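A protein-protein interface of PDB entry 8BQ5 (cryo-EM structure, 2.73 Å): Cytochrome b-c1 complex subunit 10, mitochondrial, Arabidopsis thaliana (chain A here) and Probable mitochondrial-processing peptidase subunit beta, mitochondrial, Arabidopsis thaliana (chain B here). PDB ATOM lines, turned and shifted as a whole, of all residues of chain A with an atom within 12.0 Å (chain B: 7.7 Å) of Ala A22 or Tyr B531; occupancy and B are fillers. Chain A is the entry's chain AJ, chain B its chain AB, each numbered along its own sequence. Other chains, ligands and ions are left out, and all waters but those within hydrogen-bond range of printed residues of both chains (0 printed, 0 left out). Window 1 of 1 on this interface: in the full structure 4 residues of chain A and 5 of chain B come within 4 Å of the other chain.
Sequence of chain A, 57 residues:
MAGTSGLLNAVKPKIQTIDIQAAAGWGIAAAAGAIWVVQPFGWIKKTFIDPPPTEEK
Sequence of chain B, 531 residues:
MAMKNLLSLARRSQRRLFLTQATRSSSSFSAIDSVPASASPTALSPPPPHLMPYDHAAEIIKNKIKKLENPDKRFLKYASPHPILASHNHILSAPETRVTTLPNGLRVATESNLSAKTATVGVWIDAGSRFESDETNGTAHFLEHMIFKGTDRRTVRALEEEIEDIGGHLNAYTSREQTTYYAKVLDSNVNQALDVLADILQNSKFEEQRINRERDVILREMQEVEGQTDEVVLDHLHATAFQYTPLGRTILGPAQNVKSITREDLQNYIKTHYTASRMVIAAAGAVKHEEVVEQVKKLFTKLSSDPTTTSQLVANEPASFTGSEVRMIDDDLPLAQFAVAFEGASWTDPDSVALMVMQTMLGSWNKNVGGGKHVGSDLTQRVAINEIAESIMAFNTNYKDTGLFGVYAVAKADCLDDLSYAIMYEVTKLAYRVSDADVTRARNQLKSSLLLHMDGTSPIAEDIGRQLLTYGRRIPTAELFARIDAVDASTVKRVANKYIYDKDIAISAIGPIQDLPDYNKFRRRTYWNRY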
ATOM      1  N   THR A  17      -5.562   2.733  20.463  1.00  0.00           N
ATOM      2  CA  THR A  17      -6.353   3.717  21.190  1.00  0.00           C
ATOM      3  C   THR A  17      -7.300   3.037  22.171  1.00  0.00           C
ATOM      4  O   THR A  17      -8.327   3.601  22.547  1.00  0.00           O
ATOM      5  CB  THR A  17      -7.172   4.607  20.235  1.00  0.00           C
ATOM      6  OG1 THR A  17      -8.141   3.807  19.546  1.00  0.00           O
ATOM      7  CG2 THR A  17      -6.262   5.280  19.218  1.00  0.00           C
ATOM      8  N   ILE A  18      -6.950   1.818  22.582  1.00  0.00           N
ATOM      9  CA  ILE A  18      -7.777   1.058  23.511  1.00  0.00           C
ATOM     10  C   ILE A  18      -7.227   1.092  24.936  1.00  0.00           C
ATOM     11  O   ILE A  18      -7.969   0.786  25.882  1.00  0.00           O
ATOM     12  CB  ILE A  18      -7.945  -0.396  23.019  1.00  0.00           C
ATOM     13  CG1 ILE A  18      -8.289  -0.399  21.528  1.00  0.00           C
ATOM     14  CG2 ILE A  18      -9.041  -1.118  23.788  1.00  0.00           C
ATOM     15  CD1 ILE A  18      -8.603  -1.767  20.972  1.00  0.00           C
ATOM     16  N   ASP A  19      -5.960   1.470  25.119  1.00  0.00           N
ATOM     17  CA  ASP A  19      -5.440   1.679  26.465  1.00  0.00           C
ATOM     18  C   ASP A  19      -6.175   2.815  27.165  1.00  0.00           C
ATOM     19  O   ASP A  19      -6.431   2.747  28.374  1.00  0.00           O
ATOM     20  CB  ASP A  19      -3.939   1.964  26.410  1.00  0.00           C
ATOM     21  CG  ASP A  19      -3.104   0.753  26.770  1.00  0.00           C
ATOM     22  OD1 ASP A  19      -1.885   0.913  26.987  1.00  0.00           O
ATOM     23  OD2 ASP A  19      -3.669  -0.359  26.844  1.00  0.00           O
ATOM     24  N   ILE A  20      -6.507   3.873  26.425  1.00  0.00           N
ATOM     25  CA  ILE A  20      -7.256   4.985  27.003  1.00  0.00           C
ATOM     26  C   ILE A  20      -8.647   4.531  27.427  1.00  0.00           C
ATOM     27  O   ILE A  20      -9.123   4.879  28.515  1.00  0.00           O
ATOM     28  CB  ILE A  20      -7.314   6.159  26.008  1.00  0.00           C
ATOM     29  CG1 ILE A  20      -5.923   6.773  25.834  1.00  0.00           C
ATOM     30  CG2 ILE A  20      -8.311   7.213  26.473  1.00  0.00           C
ATOM     31  CD1 ILE A  20      -5.784   7.643  24.604  1.00  0.00           C
ATOM     32  N   GLN A  21      -9.322   3.746  26.583  1.00  0.00           N
ATOM     33  CA  GLN A  21     -10.624   3.209  26.963  1.00  0.00           C
ATOM     34  C   GLN A  21     -10.498   2.237  28.129  1.00  0.00           C
ATOM     35  O   GLN A  21     -11.397   2.150  28.975  1.00  0.00           O
ATOM     36  CB  GLN A  21     -11.287   2.528  25.766  1.00  0.00           C
ATOM     37  CG  GLN A  21     -10.802   3.037  24.424  1.00  0.00           C
ATOM     38  CD  GLN A  21     -11.742   2.684  23.291  1.00  0.00           C
ATOM     39  OE1 GLN A  21     -12.905   2.350  23.516  1.00  0.00           O
ATOM     40  NE2 GLN A  21     -11.242   2.757  22.064  1.00  0.00           N
ATOM     41  N   ALA A  22      -9.395   1.488  28.184  1.00  0.00           N
ATOM     42  CA  ALA A  22      -9.153   0.618  29.330  1.00  0.00           C
ATOM     43  C   ALA A  22      -8.998   1.429  30.610  1.00  0.00           C
ATOM     44  O   ALA A  22      -9.506   1.037  31.667  1.00  0.00           O
ATOM     45  CB  ALA A  22      -7.915  -0.243  29.085  1.00  0.00           C
ATOM     46  N   ALA A  23      -8.290   2.559  30.536  1.00  0.00           N
ATOM     47  CA  ALA A  23      -8.131   3.411  31.709  1.00  0.00           C
ATOM     48  C   ALA A  23      -9.461   4.017  32.140  1.00  0.00           C
ATOM     49  O   ALA A  23      -9.776   4.055  33.336  1.00  0.00           O
ATOM     50  CB  ALA A  23      -7.109   4.512  31.425  1.00  0.00           C
ATOM     51  N   ALA A  24     -10.254   4.498  31.180  1.00  0.00           N
ATOM     52  CA  ALA A  24     -11.553   5.072  31.513  1.00  0.00           C
ATOM     53  C   ALA A  24     -12.495   4.015  32.077  1.00  0.00           C
ATOM     54  O   ALA A  24     -13.255   4.287  33.014  1.00  0.00           O
ATOM     55  CB  ALA A  24     -12.166   5.737  30.282  1.00  0.00           C
ATOM     56  N   GLY A  25     -12.463   2.805  31.516  1.00  0.00           N
ATOM     57  CA  GLY A  25     -13.304   1.739  32.036  1.00  0.00           C
ATOM     58  C   GLY A  25     -12.928   1.344  33.450  1.00  0.00           C
ATOM     59  O   GLY A  25     -13.793   1.124  34.300  1.00  0.00           O
ATOM     60  N   TRP A  26     -11.624   1.245  33.721  1.00  0.00           N
ATOM     61  CA  TRP A  26     -11.179   0.895  35.065  1.00  0.00           C
ATOM     62  C   TRP A  26     -11.378   2.048  36.041  1.00  0.00           C
ATOM     63  O   TRP A  26     -11.553   1.816  37.242  1.00  0.00           O
ATOM     64  CB  TRP A  26      -9.714   0.461  35.038  1.00  0.00           C
ATOM     65  CG  TRP A  26      -9.514  -0.950  34.566  1.00  0.00           C
ATOM     66  CD1 TRP A  26      -8.756  -1.359  33.509  1.00  0.00           C
ATOM     67  CD2 TRP A  26     -10.077  -2.138  35.139  1.00  0.00           C
ATOM     68  NE1 TRP A  26      -8.813  -2.725  33.384  1.00  0.00           N
ATOM     69  CE2 TRP A  26      -9.617  -3.228  34.373  1.00  0.00           C
ATOM     70  CE3 TRP A  26     -10.924  -2.386  36.224  1.00  0.00           C
ATOM     71  CZ2 TRP A  26      -9.976  -4.544  34.657  1.00  0.00           C
ATOM     72  CZ3 TRP A  26     -11.279  -3.693  36.502  1.00  0.00           C
ATOM     73  CH2 TRP A  26     -10.806  -4.755  35.723  1.00  0.00           C
ATOM     74  N   GLY A  27     -11.346   3.289  35.550  1.00  0.00           N
ATOM     75  CA  GLY A  27     -11.644   4.421  36.412  1.00  0.00           C
ATOM     76  C   GLY A  27     -13.082   4.420  36.891  1.00  0.00           C
ATOM     77  O   GLY A  27     -13.365   4.779  38.037  1.00  0.00           O
ATOM     78  N   ILE A  28     -14.011   4.029  36.017  1.00  0.00           N
ATOM     79  CA  ILE A  28     -15.408   3.886  36.421  1.00  0.00           C
ATOM     80  C   ILE A  28     -15.543   2.796  37.477  1.00  0.00           C
ATOM     81  O   ILE A  28     -16.272   2.954  38.464  1.00  0.00           O
ATOM     82  CB  ILE A  28     -16.295   3.610  35.190  1.00  0.00           C
ATOM     83  CG1 ILE A  28     -16.872   4.915  34.629  1.00  0.00           C
ATOM     84  CG2 ILE A  28     -17.420   2.639  35.528  1.00  0.00           C
ATOM     85  CD1 ILE A  28     -15.836   5.903  34.136  1.00  0.00           C
ATOM     86  N   ALA A  29     -14.840   1.675  37.289  1.00  0.00           N
ATOM     87  CA  ALA A  29     -14.874   0.603  38.279  1.00  0.00           C
ATOM     88  C   ALA A  29     -14.302   1.064  39.613  1.00  0.00           C
ATOM     89  O   ALA A  29     -14.849   0.744  40.675  1.00  0.00           O
ATOM     90  CB  ALA A  29     -14.111  -0.616  37.762  1.00  0.00           C
ATOM     91  N   ALA A  30     -13.196   1.810  39.580  1.00  0.00           N
ATOM     92  CA  ALA A  30     -12.618   2.329  40.816  1.00  0.00           C
ATOM     93  C   ALA A  30     -13.569   3.304  41.497  1.00  0.00           C
ATOM     94  O   ALA A  30     -13.710   3.289  42.725  1.00  0.00           O
ATOM     95  CB  ALA A  30     -11.273   2.994  40.530  1.00  0.00           C
ATOM     96  N   ALA A  31     -14.224   4.165  40.717  1.00  0.00           N
ATOM     97  CA  ALA A  31     -15.226   5.060  41.281  1.00  0.00           C
ATOM     98  C   ALA A  31     -16.418   4.279  41.820  1.00  0.00           C
ATOM     99  O   ALA A  31     -16.916   4.560  42.916  1.00  0.00           O
ATOM    100  CB  ALA A  31     -15.676   6.075  40.230  1.00  0.00           C
ATOM    101  N   TYR B 425      -1.180 -16.070  23.481  1.00  0.00           N
ATOM    102  CA  TYR B 425      -0.986 -14.637  23.688  1.00  0.00           C
ATOM    103  C   TYR B 425      -1.063 -13.874  22.373  1.00  0.00           C
ATOM    104  O   TYR B 425      -1.755 -12.856  22.272  1.00  0.00           O
ATOM    105  CB  TYR B 425       0.356 -14.379  24.373  1.00  0.00           C
ATOM    106  CG  TYR B 425       0.589 -12.926  24.715  1.00  0.00           C
ATOM    107  CD1 TYR B 425       0.102 -12.384  25.896  1.00  0.00           C
ATOM    108  CD2 TYR B 425       1.288 -12.093  23.852  1.00  0.00           C
ATOM    109  CE1 TYR B 425       0.311 -11.057  26.210  1.00  0.00           C
ATOM    110  CE2 TYR B 425       1.498 -10.764  24.156  1.00  0.00           C
ATOM    111  CZ  TYR B 425       1.007 -10.252  25.336  1.00  0.00           C
ATOM    112  OH  TYR B 425       1.217  -8.930  25.645  1.00  0.00           O
ATOM    113  N   TYR B 432      -6.976  -7.093  20.490  1.00  0.00           N
ATOM    114  CA  TYR B 432      -6.707  -5.931  21.329  1.00  0.00           C
ATOM    115  C   TYR B 432      -5.797  -4.912  20.664  1.00  0.00           C
ATOM    116  O   TYR B 432      -6.177  -3.744  20.535  1.00  0.00           O
ATOM    117  CB  TYR B 432      -6.088  -6.384  22.658  1.00  0.00           C
ATOM    118  CG  TYR B 432      -7.026  -7.179  23.532  1.00  0.00           C
ATOM    119  CD1 TYR B 432      -8.001  -6.547  24.289  1.00  0.00           C
ATOM    120  CD2 TYR B 432      -6.939  -8.562  23.596  1.00  0.00           C
ATOM    121  CE1 TYR B 432      -8.858  -7.269  25.090  1.00  0.00           C
ATOM    122  CE2 TYR B 432      -7.790  -9.292  24.393  1.00  0.00           C
ATOM    123  CZ  TYR B 432      -8.748  -8.641  25.138  1.00  0.00           C
ATOM    124  OH  TYR B 432      -9.599  -9.366  25.935  1.00  0.00           O
ATOM    125  N   ARG B 433      -4.603  -5.317  20.236  1.00  0.00           N
ATOM    126  CA  ARG B 433      -3.619  -4.399  19.672  1.00  0.00           C
ATOM    127  C   ARG B 433      -3.205  -4.899  18.296  1.00  0.00           C
ATOM    128  O   ARG B 433      -2.655  -5.998  18.172  1.00  0.00           O
ATOM    129  CB  ARG B 433      -2.402  -4.264  20.588  1.00  0.00           C
ATOM    130  CG  ARG B 433      -2.656  -3.464  21.854  1.00  0.00           C
ATOM    131  CD  ARG B 433      -2.312  -4.262  23.100  1.00  0.00           C
ATOM    132  NE  ARG B 433      -1.026  -4.940  22.984  1.00  0.00           N
ATOM    133  CZ  ARG B 433      -0.380  -5.499  23.999  1.00  0.00           C
ATOM    134  NH1 ARG B 433       0.767  -6.134  23.822  1.00  0.00           N
ATOM    135  NH2 ARG B 433      -0.897  -5.416  25.221  1.00  0.00           N
ATOM    136  N   TYR B 501     -11.963 -13.989  20.179  1.00  0.00           N
ATOM    137  CA  TYR B 501     -12.154 -13.524  21.546  1.00  0.00           C
ATOM    138  C   TYR B 501     -13.216 -14.344  22.266  1.00  0.00           C
ATOM    139  O   TYR B 501     -14.364 -14.426  21.819  1.00  0.00           O
ATOM    140  CB  TYR B 501     -12.540 -12.044  21.554  1.00  0.00           C
ATOM    141  CG  TYR B 501     -12.877 -11.525  22.930  1.00  0.00           C
ATOM    142  CD1 TYR B 501     -11.880 -11.103  23.796  1.00  0.00           C
ATOM    143  CD2 TYR B 501     -14.193 -11.465  23.370  1.00  0.00           C
ATOM    144  CE1 TYR B 501     -12.184 -10.633  25.055  1.00  0.00           C
ATOM    145  CE2 TYR B 501     -14.504 -10.998  24.628  1.00  0.00           C
ATOM    146  CZ  TYR B 501     -13.495 -10.583  25.467  1.00  0.00           C
ATOM    147  OH  TYR B 501     -13.799 -10.116  26.722  1.00  0.00           O
ATOM    148  N   TYR B 527      -8.961 -14.582  26.230  1.00  0.00           N
ATOM    149  CA  TYR B 527      -9.324 -13.215  26.565  1.00  0.00           C
ATOM    150  C   TYR B 527      -8.340 -12.683  27.596  1.00  0.00           C
ATOM    151  O   TYR B 527      -7.648 -13.443  28.277  1.00  0.00           O
ATOM    152  CB  TYR B 527     -10.763 -13.119  27.090  1.00  0.00           C
ATOM    153  CG  TYR B 527     -11.088 -14.081  28.209  1.00  0.00           C
ATOM    154  CD1 TYR B 527     -11.576 -15.351  27.939  1.00  0.00           C
ATOM    155  CD2 TYR B 527     -10.909 -13.718  29.537  1.00  0.00           C
ATOM    156  CE1 TYR B 527     -11.873 -16.233  28.956  1.00  0.00           C
ATOM    157  CE2 TYR B 527     -11.203 -14.593  30.561  1.00  0.00           C
ATOM    158  CZ  TYR B 527     -11.685 -15.848  30.265  1.00  0.00           C
ATOM    159  OH  TYR B 527     -11.981 -16.722  31.283  1.00  0.00           O
ATOM    160  N   TRP B 528      -8.277 -11.359  27.701  1.00  0.00           N
ATOM    161  CA  TRP B 528      -7.417 -10.680  28.661  1.00  0.00           C
ATOM    162  C   TRP B 528      -8.296  -9.973  29.681  1.00  0.00           C
ATOM    163  O   TRP B 528      -9.154  -9.166  29.310  1.00  0.00           O
ATOM    164  CB  TRP B 528      -6.491  -9.682  27.963  1.00  0.00           C
ATOM    165  CG  TRP B 528      -5.432 -10.330  27.130  1.00  0.00           C
ATOM    166  CD1 TRP B 528      -5.122 -11.656  27.086  1.00  0.00           C
ATOM    167  CD2 TRP B 528      -4.543  -9.680  26.217  1.00  0.00           C
ATOM    168  NE1 TRP B 528      -4.093 -11.872  26.203  1.00  0.00           N
ATOM    169  CE2 TRP B 528      -3.720 -10.674  25.656  1.00  0.00           C
ATOM    170  CE3 TRP B 528      -4.362  -8.351  25.820  1.00  0.00           C
ATOM    171  CZ2 TRP B 528      -2.733 -10.384  24.720  1.00  0.00           C
ATOM    172  CZ3 TRP B 528      -3.382  -8.065  24.890  1.00  0.00           C
ATOM    173  CH2 TRP B 528      -2.580  -9.077  24.351  1.00  0.00           C
ATOM    174  N   ASN B 529      -8.080 -10.271  30.961  1.00  0.00           N
ATOM    175  CA  ASN B 529      -8.903  -9.691  32.013  1.00  0.00           C
ATOM    176  C   ASN B 529      -8.449  -8.299  32.424  1.00  0.00           C
ATOM    177  O   ASN B 529      -9.138  -7.652  33.221  1.00  0.00           O
ATOM    178  CB  ASN B 529      -8.923 -10.613  33.233  1.00  0.00           C
ATOM    179  CG  ASN B 529     -10.157 -11.490  33.276  1.00  0.00           C
ATOM    180  OD1 ASN B 529     -11.121 -11.256  32.549  1.00  0.00           O
ATOM    181  ND2 ASN B 529     -10.131 -12.509  34.124  1.00  0.00           N
ATOM    182  N   ARG B 530      -7.320  -7.820  31.908  1.00  0.00           N
ATOM    183  CA  ARG B 530      -6.871  -6.463  32.187  1.00  0.00           C
ATOM    184  C   ARG B 530      -7.525  -5.429  31.282  1.00  0.00           C
ATOM    185  O   ARG B 530      -7.278  -4.231  31.457  1.00  0.00           O
ATOM    186  CB  ARG B 530      -5.349  -6.373  32.057  1.00  0.00           C
ATOM    187  CG  ARG B 530      -4.833  -6.545  30.641  1.00  0.00           C
ATOM    188  CD  ARG B 530      -3.325  -6.696  30.635  1.00  0.00           C
ATOM    189  NE  ARG B 530      -2.811  -7.045  29.317  1.00  0.00           N
ATOM    190  CZ  ARG B 530      -2.265  -8.213  29.012  1.00  0.00           C
ATOM    191  NH1 ARG B 530      -2.165  -9.183  29.906  1.00  0.00           N
ATOM    192  NH2 ARG B 530      -1.807  -8.415  27.781  1.00  0.00           N
ATOM    193  N   TYR B 531      -8.342  -5.858  30.325  1.00  0.00           N
ATOM    194  CA  TYR B 531      -9.066  -4.936  29.460  1.00  0.00           C
ATOM    195  C   TYR B 531     -10.567  -5.055  29.692  1.00  0.00           C
ATOM    196  O   TYR B 531     -11.074  -4.659  30.740  1.00  0.00           O
ATOM    197  CB  TYR B 531      -8.738  -5.200  27.989  1.00  0.00           C
ATOM    198  CG  TYR B 531      -7.372  -4.717  27.566  1.00  0.00           C
ATOM    199  CD1 TYR B 531      -7.132  -3.370  27.333  1.00  0.00           C
ATOM    200  CD2 TYR B 531      -6.322  -5.608  27.395  1.00  0.00           C
ATOM    201  CE1 TYR B 531      -5.884  -2.923  26.945  1.00  0.00           C
ATOM    202  CE2 TYR B 531      -5.071  -5.170  27.008  1.00  0.00           C
ATOM    203  CZ  TYR B 531      -4.858  -3.827  26.785  1.00  0.00           C
ATOM    204  OH  TYR B 531      -3.613  -3.386  26.397  1.00  0.00           O
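N of Trp B528 lies within hydrogen-bond range of OH of Tyr B432 (3.0 Å).
Printed residues of chain B within 4 Å of Asp A19: Tyr B531.
Ala A22 touches just one residue of chain B: Tyr B531.
Ala A24 touches none of the printed residues of chain B.
Printed residues of chain B within 4 Å of Trp A26: Asn B529 (3.5 Å), Arg B530 (2.9 Å) and Tyr B531 (3.98 Å).
Tyr B432 touches just one residue of chain A: Ile A18 (3.2 Å).
Asn B529 touches just one residue of chain A: Trp A26 (3.5 Å).
Of the printed residues of chain A, Tyr B531 touches Asp A19, Ala A22 and Trp A26.
The nearest printed residue of chain B that does not touch Ile A18 is Tyr B531 (4.4 Å).
Ile A18 touches Tyr B432.
Tyr B531 touches Ala A22 (CD1 to CB, 3.7 Å).
Trp A26 touches Asn B529 (CZ2 to O, 3.5 Å).
Trp A26 touches Tyr B531.
Of the 15 printed residues of chain A, 4 touch a printed residue of chain B.
Hydrophobic or aromatic side chains of chain A that line the printed part of chain B: Ile A18, Ala A22 and Trp A26.
Along chain A the printed residues that touch a printed residue of chain B span positions 18 to 26.
Hydrophobic or aromatic side chains of chain B that line the printed part of chain A: Tyr B531.
The indole nitrogen (NE1) of Trp A26 is in hydrogen-bond range of the backbone carbonyl oxygen (O) of Arg B530 (2.9 Å).
OH of Tyr B531 is in hydrogen-bond range of OD2 of Asp A19 (3.1 Å).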
